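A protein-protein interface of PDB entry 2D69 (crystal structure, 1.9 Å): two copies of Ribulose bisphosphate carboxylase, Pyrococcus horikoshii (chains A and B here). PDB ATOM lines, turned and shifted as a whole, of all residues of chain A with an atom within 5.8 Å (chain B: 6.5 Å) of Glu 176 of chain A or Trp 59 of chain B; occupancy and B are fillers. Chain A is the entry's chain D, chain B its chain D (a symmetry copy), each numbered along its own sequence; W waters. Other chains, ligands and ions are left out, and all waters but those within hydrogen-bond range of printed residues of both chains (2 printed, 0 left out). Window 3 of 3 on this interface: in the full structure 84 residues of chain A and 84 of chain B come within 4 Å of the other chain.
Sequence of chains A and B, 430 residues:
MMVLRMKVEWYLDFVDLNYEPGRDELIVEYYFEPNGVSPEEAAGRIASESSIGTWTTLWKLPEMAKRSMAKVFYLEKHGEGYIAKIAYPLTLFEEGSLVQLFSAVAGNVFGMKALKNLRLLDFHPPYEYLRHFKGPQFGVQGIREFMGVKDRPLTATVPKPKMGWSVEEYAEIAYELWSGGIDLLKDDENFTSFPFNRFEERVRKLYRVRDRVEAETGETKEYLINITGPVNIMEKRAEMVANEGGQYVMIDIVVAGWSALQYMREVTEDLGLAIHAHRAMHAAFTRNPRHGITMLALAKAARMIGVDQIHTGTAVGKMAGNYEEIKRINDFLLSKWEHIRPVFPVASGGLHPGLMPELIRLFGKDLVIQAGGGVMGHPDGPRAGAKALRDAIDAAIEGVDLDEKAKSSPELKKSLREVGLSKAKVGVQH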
ATOM      1  N   TRP A 165      -5.877   8.273 -15.762  1.00  0.00           N
ATOM      2  CA  TRP A 165      -5.060   9.071 -16.670  1.00  0.00           C
ATOM      3  C   TRP A 165      -4.738  10.448 -16.079  1.00  0.00           C
ATOM      4  O   TRP A 165      -5.626  11.129 -15.614  1.00  0.00           O
ATOM      5  CB  TRP A 165      -5.844   9.343 -17.949  1.00  0.00           C
ATOM      6  CG  TRP A 165      -6.361   8.156 -18.627  1.00  0.00           C
ATOM      7  CD1 TRP A 165      -7.565   7.566 -18.428  1.00  0.00           C
ATOM      8  CD2 TRP A 165      -5.720   7.432 -19.663  1.00  0.00           C
ATOM      9  NE1 TRP A 165      -7.708   6.489 -19.256  1.00  0.00           N
ATOM     10  CE2 TRP A 165      -6.583   6.375 -20.029  1.00  0.00           C
ATOM     11  CE3 TRP A 165      -4.482   7.542 -20.311  1.00  0.00           C
ATOM     12  CZ2 TRP A 165      -6.258   5.455 -21.007  1.00  0.00           C
ATOM     13  CZ3 TRP A 165      -4.168   6.643 -21.271  1.00  0.00           C
ATOM     14  CH2 TRP A 165      -5.036   5.587 -21.610  1.00  0.00           C
ATOM     15  N   GLU A 169      -1.220  12.312 -19.989  1.00  0.00           N
ATOM     16  CA  GLU A 169      -1.432  10.958 -20.495  1.00  0.00           C
ATOM     17  C   GLU A 169      -2.723  10.948 -21.315  1.00  0.00           C
ATOM     18  O   GLU A 169      -2.760  10.377 -22.396  1.00  0.00           O
ATOM     19  CB  GLU A 169      -1.492   9.925 -19.365  1.00  0.00           C
ATOM     20  CG  GLU A 169      -0.176   9.665 -18.614  1.00  0.00           C
ATOM     21  CD  GLU A 169      -0.379   8.862 -17.345  1.00  0.00           C
ATOM     22  OE1 GLU A 169      -1.485   8.945 -16.718  1.00  0.00           O
ATOM     23  OE2 GLU A 169       0.559   8.127 -16.964  1.00  0.00           O
ATOM     24  N   ALA A 171      -4.160  13.636 -22.839  1.00  0.00           N
ATOM     25  CA  ALA A 171      -3.819  14.377 -24.081  1.00  0.00           C
ATOM     26  C   ALA A 171      -3.144  13.506 -25.111  1.00  0.00           C
ATOM     27  O   ALA A 171      -3.418  13.610 -26.318  1.00  0.00           O
ATOM     28  CB  ALA A 171      -2.957  15.563 -23.760  1.00  0.00           C
ATOM     29  N   GLU A 172      -2.253  12.648 -24.673  1.00  0.00           N
ATOM     30  CA  GLU A 172      -1.488  11.856 -25.645  1.00  0.00           C
ATOM     31  C   GLU A 172      -2.372  10.772 -26.269  1.00  0.00           C
ATOM     32  O   GLU A 172      -2.317  10.561 -27.467  1.00  0.00           O
ATOM     33  CB  GLU A 172      -0.267  11.259 -24.998  1.00  0.00           C
ATOM     34  CG  GLU A 172       0.849  12.284 -24.829  1.00  0.00           C
ATOM     35  CD  GLU A 172       2.059  11.700 -24.111  1.00  0.00           C
ATOM     36  OE1 GLU A 172       2.405  10.525 -24.375  1.00  0.00           O
ATOM     37  OE2 GLU A 172       2.674  12.424 -23.299  1.00  0.00           O
ATOM     38  N   ILE A 173      -3.277  10.160 -25.472  1.00  0.00           N
ATOM     39  CA  ILE A 173      -4.140   9.123 -26.030  1.00  0.00           C
ATOM     40  C   ILE A 173      -5.168   9.778 -26.955  1.00  0.00           C
ATOM     41  O   ILE A 173      -5.392   9.298 -28.074  1.00  0.00           O
ATOM     42  CB  ILE A 173      -4.722   8.147 -24.947  1.00  0.00           C
ATOM     43  CG1 ILE A 173      -5.496   6.976 -25.598  1.00  0.00           C
ATOM     44  CG2 ILE A 173      -5.632   8.891 -23.901  1.00  0.00           C
ATOM     45  CD1 ILE A 173      -4.639   6.111 -26.520  1.00  0.00           C
ATOM     46  N   ALA A 174      -5.716  10.920 -26.531  1.00  0.00           N
ATOM     47  CA  ALA A 174      -6.665  11.706 -27.330  1.00  0.00           C
ATOM     48  C   ALA A 174      -6.122  12.039 -28.699  1.00  0.00           C
ATOM     49  O   ALA A 174      -6.838  11.913 -29.693  1.00  0.00           O
ATOM     50  CB  ALA A 174      -6.997  12.993 -26.633  1.00  0.00           C
ATOM     51  N   TYR A 175      -4.879  12.503 -28.744  1.00  0.00           N
ATOM     52  CA  TYR A 175      -4.237  12.828 -30.025  1.00  0.00           C
ATOM     53  C   TYR A 175      -4.171  11.628 -30.965  1.00  0.00           C
ATOM     54  O   TYR A 175      -4.369  11.769 -32.181  1.00  0.00           O
ATOM     55  CB  TYR A 175      -2.830  13.360 -29.799  1.00  0.00           C
ATOM     56  CG  TYR A 175      -2.137  13.789 -31.078  1.00  0.00           C
ATOM     57  CD1 TYR A 175      -1.209  12.963 -31.704  1.00  0.00           C
ATOM     58  CD2 TYR A 175      -2.428  15.004 -31.669  1.00  0.00           C
ATOM     59  CE1 TYR A 175      -0.590  13.356 -32.901  1.00  0.00           C
ATOM     60  CE2 TYR A 175      -1.816  15.401 -32.867  1.00  0.00           C
ATOM     61  CZ  TYR A 175      -0.885  14.582 -33.464  1.00  0.00           C
ATOM     62  OH  TYR A 175      -0.289  15.032 -34.649  1.00  0.00           O
ATOM     63  N   GLU A 176      -3.810  10.468 -30.420  1.00  0.00           N
ATOM     64  CA  GLU A 176      -3.830   9.234 -31.200  1.00  0.00           C
ATOM     65  C   GLU A 176      -5.225   8.948 -31.760  1.00  0.00           C
ATOM     66  O   GLU A 176      -5.398   8.721 -32.943  1.00  0.00           O
ATOM     67  CB  GLU A 176      -3.392   8.020 -30.367  1.00  0.00           C
ATOM     68  CG  GLU A 176      -1.958   8.049 -29.960  1.00  0.00           C
ATOM     69  CD  GLU A 176      -1.068   8.319 -31.144  1.00  0.00           C
ATOM     70  OE1 GLU A 176      -0.408   9.369 -31.146  1.00  0.00           O
ATOM     71  OE2 GLU A 176      -1.035   7.491 -32.065  1.00  0.00           O
ATOM     72  N   LEU A 177      -6.226   9.007 -30.919  1.00  0.00           N
ATOM     73  CA  LEU A 177      -7.555   8.616 -31.335  1.00  0.00           C
ATOM     74  C   LEU A 177      -8.123   9.562 -32.375  1.00  0.00           C
ATOM     75  O   LEU A 177      -8.652   9.103 -33.379  1.00  0.00           O
ATOM     76  CB  LEU A 177      -8.483   8.565 -30.123  1.00  0.00           C
ATOM     77  CG  LEU A 177      -8.182   7.416 -29.162  1.00  0.00           C
ATOM     78  CD1 LEU A 177      -9.050   7.580 -27.858  1.00  0.00           C
ATOM     79  CD2 LEU A 177      -8.465   6.130 -29.800  1.00  0.00           C
ATOM     80  N   TRP A 178      -8.106  10.871 -32.083  1.00  0.00           N
ATOM     81  CA  TRP A 178      -8.582  11.902 -32.997  1.00  0.00           C
ATOM     82  C   TRP A 178      -7.797  11.840 -34.328  1.00  0.00           C
ATOM     83  O   TRP A 178      -8.420  11.880 -35.396  1.00  0.00           O
ATOM     84  CB  TRP A 178      -8.445  13.291 -32.369  1.00  0.00           C
ATOM     85  CG  TRP A 178      -9.554  13.724 -31.458  1.00  0.00           C
ATOM     86  CD1 TRP A 178     -10.889  13.455 -31.583  1.00  0.00           C
ATOM     87  CD2 TRP A 178      -9.426  14.557 -30.295  1.00  0.00           C
ATOM     88  NE1 TRP A 178     -11.592  14.085 -30.590  1.00  0.00           N
ATOM     89  CE2 TRP A 178     -10.723  14.769 -29.782  1.00  0.00           C
ATOM     90  CE3 TRP A 178      -8.338  15.180 -29.654  1.00  0.00           C
ATOM     91  CZ2 TRP A 178     -10.967  15.530 -28.651  1.00  0.00           C
ATOM     92  CZ3 TRP A 178      -8.575  15.953 -28.527  1.00  0.00           C
ATOM     93  CH2 TRP A 178      -9.882  16.098 -28.018  1.00  0.00           C
ATOM     94  N   SER A 179      -6.475  11.712 -34.281  1.00  0.00           N
ATOM     95  CA  SER A 179      -5.686  11.749 -35.522  1.00  0.00           C
ATOM     96  C   SER A 179      -5.931  10.546 -36.425  1.00  0.00           C
ATOM     97  O   SER A 179      -5.733  10.624 -37.641  1.00  0.00           O
ATOM     98  CB  SER A 179      -4.147  11.830 -35.282  1.00  0.00           C
ATOM     99  OG  SER A 179      -3.802  12.841 -34.339  1.00  0.00           O
ATOM    100  N   GLY A 180      -6.290   9.415 -35.831  1.00  0.00           N
ATOM    101  CA  GLY A 180      -6.487   8.195 -36.602  1.00  0.00           C
ATOM    102  C   GLY A 180      -7.867   8.195 -37.216  1.00  0.00           C
ATOM    103  O   GLY A 180      -8.150   7.414 -38.099  1.00  0.00           O
ATOM    104  N   GLY A 181      -8.736   9.088 -36.755  1.00  0.00           N
ATOM    105  CA  GLY A 181     -10.029   9.267 -37.392  1.00  0.00           C
ATOM    106  C   GLY A 181     -11.266   9.350 -36.498  1.00  0.00           C
ATOM    107  O   GLY A 181     -12.357   9.579 -37.019  1.00  0.00           O
ATOM    108  N   MET A 376      -9.050   0.745 -29.066  1.00  0.00           N
ATOM    109  CA  MET A 376      -7.888   0.695 -28.181  1.00  0.00           C
ATOM    110  C   MET A 376      -7.107  -0.592 -28.379  1.00  0.00           C
ATOM    111  O   MET A 376      -5.912  -0.596 -28.167  1.00  0.00           O
ATOM    112  CB  MET A 376      -8.234   0.824 -26.709  1.00  0.00           C
ATOM    113  CG  MET A 376      -8.774   2.243 -26.280  1.00  0.00           C
ATOM    114  SD  MET A 376      -7.596   3.556 -26.496  1.00  0.00           S
ATOM    115  CE  MET A 376      -6.317   3.087 -25.351  1.00  0.00           C
ATOM    116  N   GLY A 381      -2.045  -0.440 -32.499  1.00  0.00           N
ATOM    117  CA  GLY A 381      -2.349   0.681 -31.580  1.00  0.00           C
ATOM    118  C   GLY A 381      -3.619   1.437 -31.885  1.00  0.00           C
ATOM    119  O   GLY A 381      -4.244   1.178 -32.902  1.00  0.00           O
ATOM    120  N   PRO A 382      -4.007   2.352 -30.981  1.00  0.00           N
ATOM    121  CA  PRO A 382      -5.284   3.079 -31.031  1.00  0.00           C
ATOM    122  C   PRO A 382      -5.523   3.868 -32.315  1.00  0.00           C
ATOM    123  O   PRO A 382      -6.609   3.972 -32.831  1.00  0.00           O
ATOM    124  CB  PRO A 382      -5.163   4.066 -29.861  1.00  0.00           C
ATOM    125  CG  PRO A 382      -4.207   3.476 -28.935  1.00  0.00           C
ATOM    126  CD  PRO A 382      -3.208   2.709 -29.790  1.00  0.00           C
ATOM    127  N   ARG A 383      -4.476   4.487 -32.795  1.00  0.00           N
ATOM    128  CA  ARG A 383      -4.573   5.318 -33.964  1.00  0.00           C
ATOM    129  C   ARG A 383      -4.938   4.457 -35.162  1.00  0.00           C
ATOM    130  O   ARG A 383      -5.823   4.808 -35.949  1.00  0.00           O
ATOM    131  CB  ARG A 383      -3.222   5.946 -34.157  1.00  0.00           C
ATOM    132  CG  ARG A 383      -3.076   6.947 -35.248  1.00  0.00           C
ATOM    133  CD  ARG A 383      -1.929   7.810 -34.876  1.00  0.00           C
ATOM    134  NE  ARG A 383      -1.578   8.802 -35.822  1.00  0.00           N
ATOM    135  CZ  ARG A 383      -0.648   9.693 -35.581  1.00  0.00           C
ATOM    136  NH1 ARG A 383       0.001   9.700 -34.405  1.00  0.00           N
ATOM    137  NH2 ARG A 383      -0.347  10.572 -36.519  1.00  0.00           N
ATOM    138  N   ALA A 386      -8.634   3.407 -34.878  1.00  0.00           N
ATOM    139  CA  ALA A 386      -9.577   4.473 -35.252  1.00  0.00           C
ATOM    140  C   ALA A 386      -9.711   4.484 -36.765  1.00  0.00           C
ATOM    141  O   ALA A 386     -10.829   4.553 -37.262  1.00  0.00           O
ATOM    142  CB  ALA A 386      -9.105   5.862 -34.755  1.00  0.00           C
ATOM    143  N   LEU B   4      -4.190  -8.631 -29.331  1.00  0.00           N
ATOM    144  CA  LEU B   4      -4.007  -8.287 -27.934  1.00  0.00           C
ATOM    145  C   LEU B   4      -5.121  -8.838 -27.066  1.00  0.00           C
ATOM    146  O   LEU B   4      -6.269  -8.798 -27.440  1.00  0.00           O
ATOM    147  CB  LEU B   4      -3.889  -6.794 -27.772  1.00  0.00           C
ATOM    148  CG  LEU B   4      -2.775  -6.107 -28.541  1.00  0.00           C
ATOM    149  CD1 LEU B   4      -2.771  -4.673 -28.157  1.00  0.00           C
ATOM    150  CD2 LEU B   4      -1.385  -6.707 -28.241  1.00  0.00           C
ATOM    151  N   TRP B  55      -8.121  -3.256 -20.019  1.00  0.00           N
ATOM    152  CA  TRP B  55      -6.868  -2.652 -20.464  1.00  0.00           C
ATOM    153  C   TRP B  55      -6.208  -3.346 -21.637  1.00  0.00           C
ATOM    154  O   TRP B  55      -4.973  -3.333 -21.724  1.00  0.00           O
ATOM    155  CB  TRP B  55      -5.851  -2.633 -19.290  1.00  0.00           C
ATOM    156  CG  TRP B  55      -5.507  -3.955 -18.759  1.00  0.00           C
ATOM    157  CD1 TRP B  55      -4.514  -4.811 -19.213  1.00  0.00           C
ATOM    158  CD2 TRP B  55      -6.145  -4.632 -17.679  1.00  0.00           C
ATOM    159  NE1 TRP B  55      -4.519  -5.973 -18.478  1.00  0.00           N
ATOM    160  CE2 TRP B  55      -5.505  -5.892 -17.527  1.00  0.00           C
ATOM    161  CE3 TRP B  55      -7.207  -4.313 -16.827  1.00  0.00           C
ATOM    162  CZ2 TRP B  55      -5.882  -6.816 -16.555  1.00  0.00           C
ATOM    163  CZ3 TRP B  55      -7.591  -5.244 -15.862  1.00  0.00           C
ATOM    164  CH2 TRP B  55      -6.932  -6.489 -15.747  1.00  0.00           C
ATOM    165  N   THR B  57      -4.740  -3.232 -24.593  1.00  0.00           N
ATOM    166  CA  THR B  57      -4.197  -2.300 -25.554  1.00  0.00           C
ATOM    167  C   THR B  57      -2.689  -2.348 -25.507  1.00  0.00           C
ATOM    168  O   THR B  57      -2.094  -2.778 -24.522  1.00  0.00           O
ATOM    169  CB  THR B  57      -4.676  -0.825 -25.263  1.00  0.00           C
ATOM    170  OG1 THR B  57      -4.049   0.076 -26.182  1.00  0.00           O
ATOM    171  CG2 THR B  57      -4.205  -0.304 -23.884  1.00  0.00           C
ATOM    172  N   LEU B  58      -2.088  -1.857 -26.581  1.00  0.00           N
ATOM    173  CA  LEU B  58      -0.650  -1.712 -26.669  1.00  0.00           C
ATOM    174  C   LEU B  58      -0.243  -0.344 -26.055  1.00  0.00           C
ATOM    175  O   LEU B  58       0.882  -0.128 -25.638  1.00  0.00           O
ATOM    176  CB  LEU B  58      -0.263  -1.775 -28.161  1.00  0.00           C
ATOM    177  CG  LEU B  58       1.059  -2.369 -28.552  1.00  0.00           C
ATOM    178  CD1 LEU B  58       1.303  -2.101 -30.056  1.00  0.00           C
ATOM    179  CD2 LEU B  58       2.160  -1.769 -27.637  1.00  0.00           C
ATOM    180  N   TRP B  59      -1.168   0.605 -26.021  1.00  0.00           N
ATOM    181  CA  TRP B  59      -0.840   1.940 -25.490  1.00  0.00           C
ATOM    182  C   TRP B  59      -0.402   1.917 -24.025  1.00  0.00           C
ATOM    183  O   TRP B  59      -1.003   1.188 -23.208  1.00  0.00           O
ATOM    184  CB  TRP B  59      -2.048   2.881 -25.567  1.00  0.00           C
ATOM    185  CG  TRP B  59      -1.645   4.284 -25.446  1.00  0.00           C
ATOM    186  CD1 TRP B  59      -1.878   5.111 -24.382  1.00  0.00           C
ATOM    187  CD2 TRP B  59      -0.923   5.067 -26.422  1.00  0.00           C
ATOM    188  NE1 TRP B  59      -1.333   6.348 -24.636  1.00  0.00           N
ATOM    189  CE2 TRP B  59      -0.730   6.343 -25.871  1.00  0.00           C
ATOM    190  CE3 TRP B  59      -0.387   4.796 -27.699  1.00  0.00           C
ATOM    191  CZ2 TRP B  59      -0.053   7.357 -26.542  1.00  0.00           C
ATOM    192  CZ3 TRP B  59       0.292   5.805 -28.375  1.00  0.00           C
ATOM    193  CH2 TRP B  59       0.452   7.075 -27.797  1.00  0.00           C
ATOM    194  N   LYS B  60       0.596   2.730 -23.691  1.00  0.00           N
ATOM    195  CA  LYS B  60       1.109   2.751 -22.318  1.00  0.00           C
ATOM    196  C   LYS B  60      -0.001   2.978 -21.368  1.00  0.00           C
ATOM    197  O   LYS B  60      -0.765   3.918 -21.585  1.00  0.00           O
ATOM    198  CB  LYS B  60       2.106   3.895 -22.112  1.00  0.00           C
ATOM    199  CG  LYS B  60       3.109   3.605 -20.983  1.00  0.00           C
ATOM    200  CD  LYS B  60       3.891   4.858 -20.512  1.00  0.00           C
ATOM    201  CE  LYS B  60       4.310   4.709 -19.016  1.00  0.00           C
ATOM    202  NZ  LYS B  60       3.138   4.749 -18.060  1.00  0.00           N
ATOM    203  N   LEU B  61      -0.070   2.188 -20.289  1.00  0.00           N
ATOM    204  CA  LEU B  61      -1.118   2.350 -19.300  1.00  0.00           C
ATOM    205  C   LEU B  61      -0.851   3.531 -18.350  1.00  0.00           C
ATOM    206  O   LEU B  61       0.288   3.767 -17.965  1.00  0.00           O
ATOM    207  CB  LEU B  61      -1.301   1.060 -18.471  1.00  0.00           C
ATOM    208  CG  LEU B  61      -1.323  -0.237 -19.292  1.00  0.00           C
ATOM    209  CD1 LEU B  61      -1.508  -1.378 -18.363  1.00  0.00           C
ATOM    210  CD2 LEU B  61      -2.413  -0.229 -20.375  1.00  0.00           C
ATOM    211  N   PRO B  62      -1.901   4.261 -17.972  1.00  0.00           N
ATOM    212  CA  PRO B  62      -1.745   5.438 -17.094  1.00  0.00           C
ATOM    213  C   PRO B  62      -1.178   5.059 -15.738  1.00  0.00           C
ATOM    214  O   PRO B  62      -1.584   4.025 -15.210  1.00  0.00           O
ATOM    215  CB  PRO B  62      -3.181   5.974 -16.925  1.00  0.00           C
ATOM    216  CG  PRO B  62      -4.082   5.002 -17.537  1.00  0.00           C
ATOM    217  CD  PRO B  62      -3.302   4.050 -18.370  1.00  0.00           C
HETATM  218  O   HOH W   1       1.740   6.640 -18.823  1.00  0.00           O
HETATM  219  O   HOH W   2      -3.701  -1.593 -28.995  1.00  0.00           O
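Among the printed residues, merely in contact across the chains: Trp 165 of chain A with Pro 62 of chain B (3.6 Å), Glu 169 of chain A with Pro 62 of chain B (3.4 Å), Ile 173 of chain A with Trp 59 of chain B (3.6 Å) and Glu 176 of chain A with Trp 59 of chain B (3.4 Å).
Glu 176 of chain A touches just one residue of chain B: Trp 59.
Of the printed residues of chain B, Met 376 of chain A touches Thr 57.
Printed residues of chain B within 4 Å of Trp 165 of chain A: Pro 62 (3.6 Å).
Leu 4 of chain B touches none of the printed residues of chain A.
The nearest printed residue of chain B that does not touch Ile 173 of chain A is Thr 57 of chain B (6.1 Å).
N of Trp 59 of chain B is in hydrogen-bond range of OG1 of Thr 57 of chain B, 2.9 Å away.
The side-chain carboxylate of Glu 176 of chain A lies within salt-bridge range of the guanidinium group of Arg 383 of chain A (3.3 Å).
Water W1 lies within hydrogen-bond range of NZ of Lys 60 of chain B (2.5 Å), OE2 of Glu 169 of chain A (2.7 Å) and O of Leu 61 of chain B (3.3 Å).
Water W2 lies within hydrogen-bond range of the backbone carbonyl oxygen (O) of Met 376 of chain A (2.6 Å), the backbone NH (N) of Leu 58 of chain B (2.9 Å) and the side-chain hydroxyl (OG1) of Thr 57 of chain B (3.3 Å).
Printed residues of chain A that touch a printed residue of chain B: Trp 165, Glu 169, Ile 173, Glu 176 and Met 376.
Hydrophobic or aromatic side chains of chain A that line the printed part of chain B: Trp 165, Ile 173 and Met 376.
Among the printed residues, 5 pairs touch across the chains.
Among the printed residues, no Asp or Glu carboxylate lies within 4 Å of a Lys or Arg side-chain nitrogen of the other chain.
OG1 of Thr 57 of chain B lies within hydrogen-bond range of O of Met 376 of chain A, at 2.8 Å.
No position is printed for both chains.
Of the 5 pairs that touch across the chains among the printed residues, none has its exchanged pair printed and touching as well.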
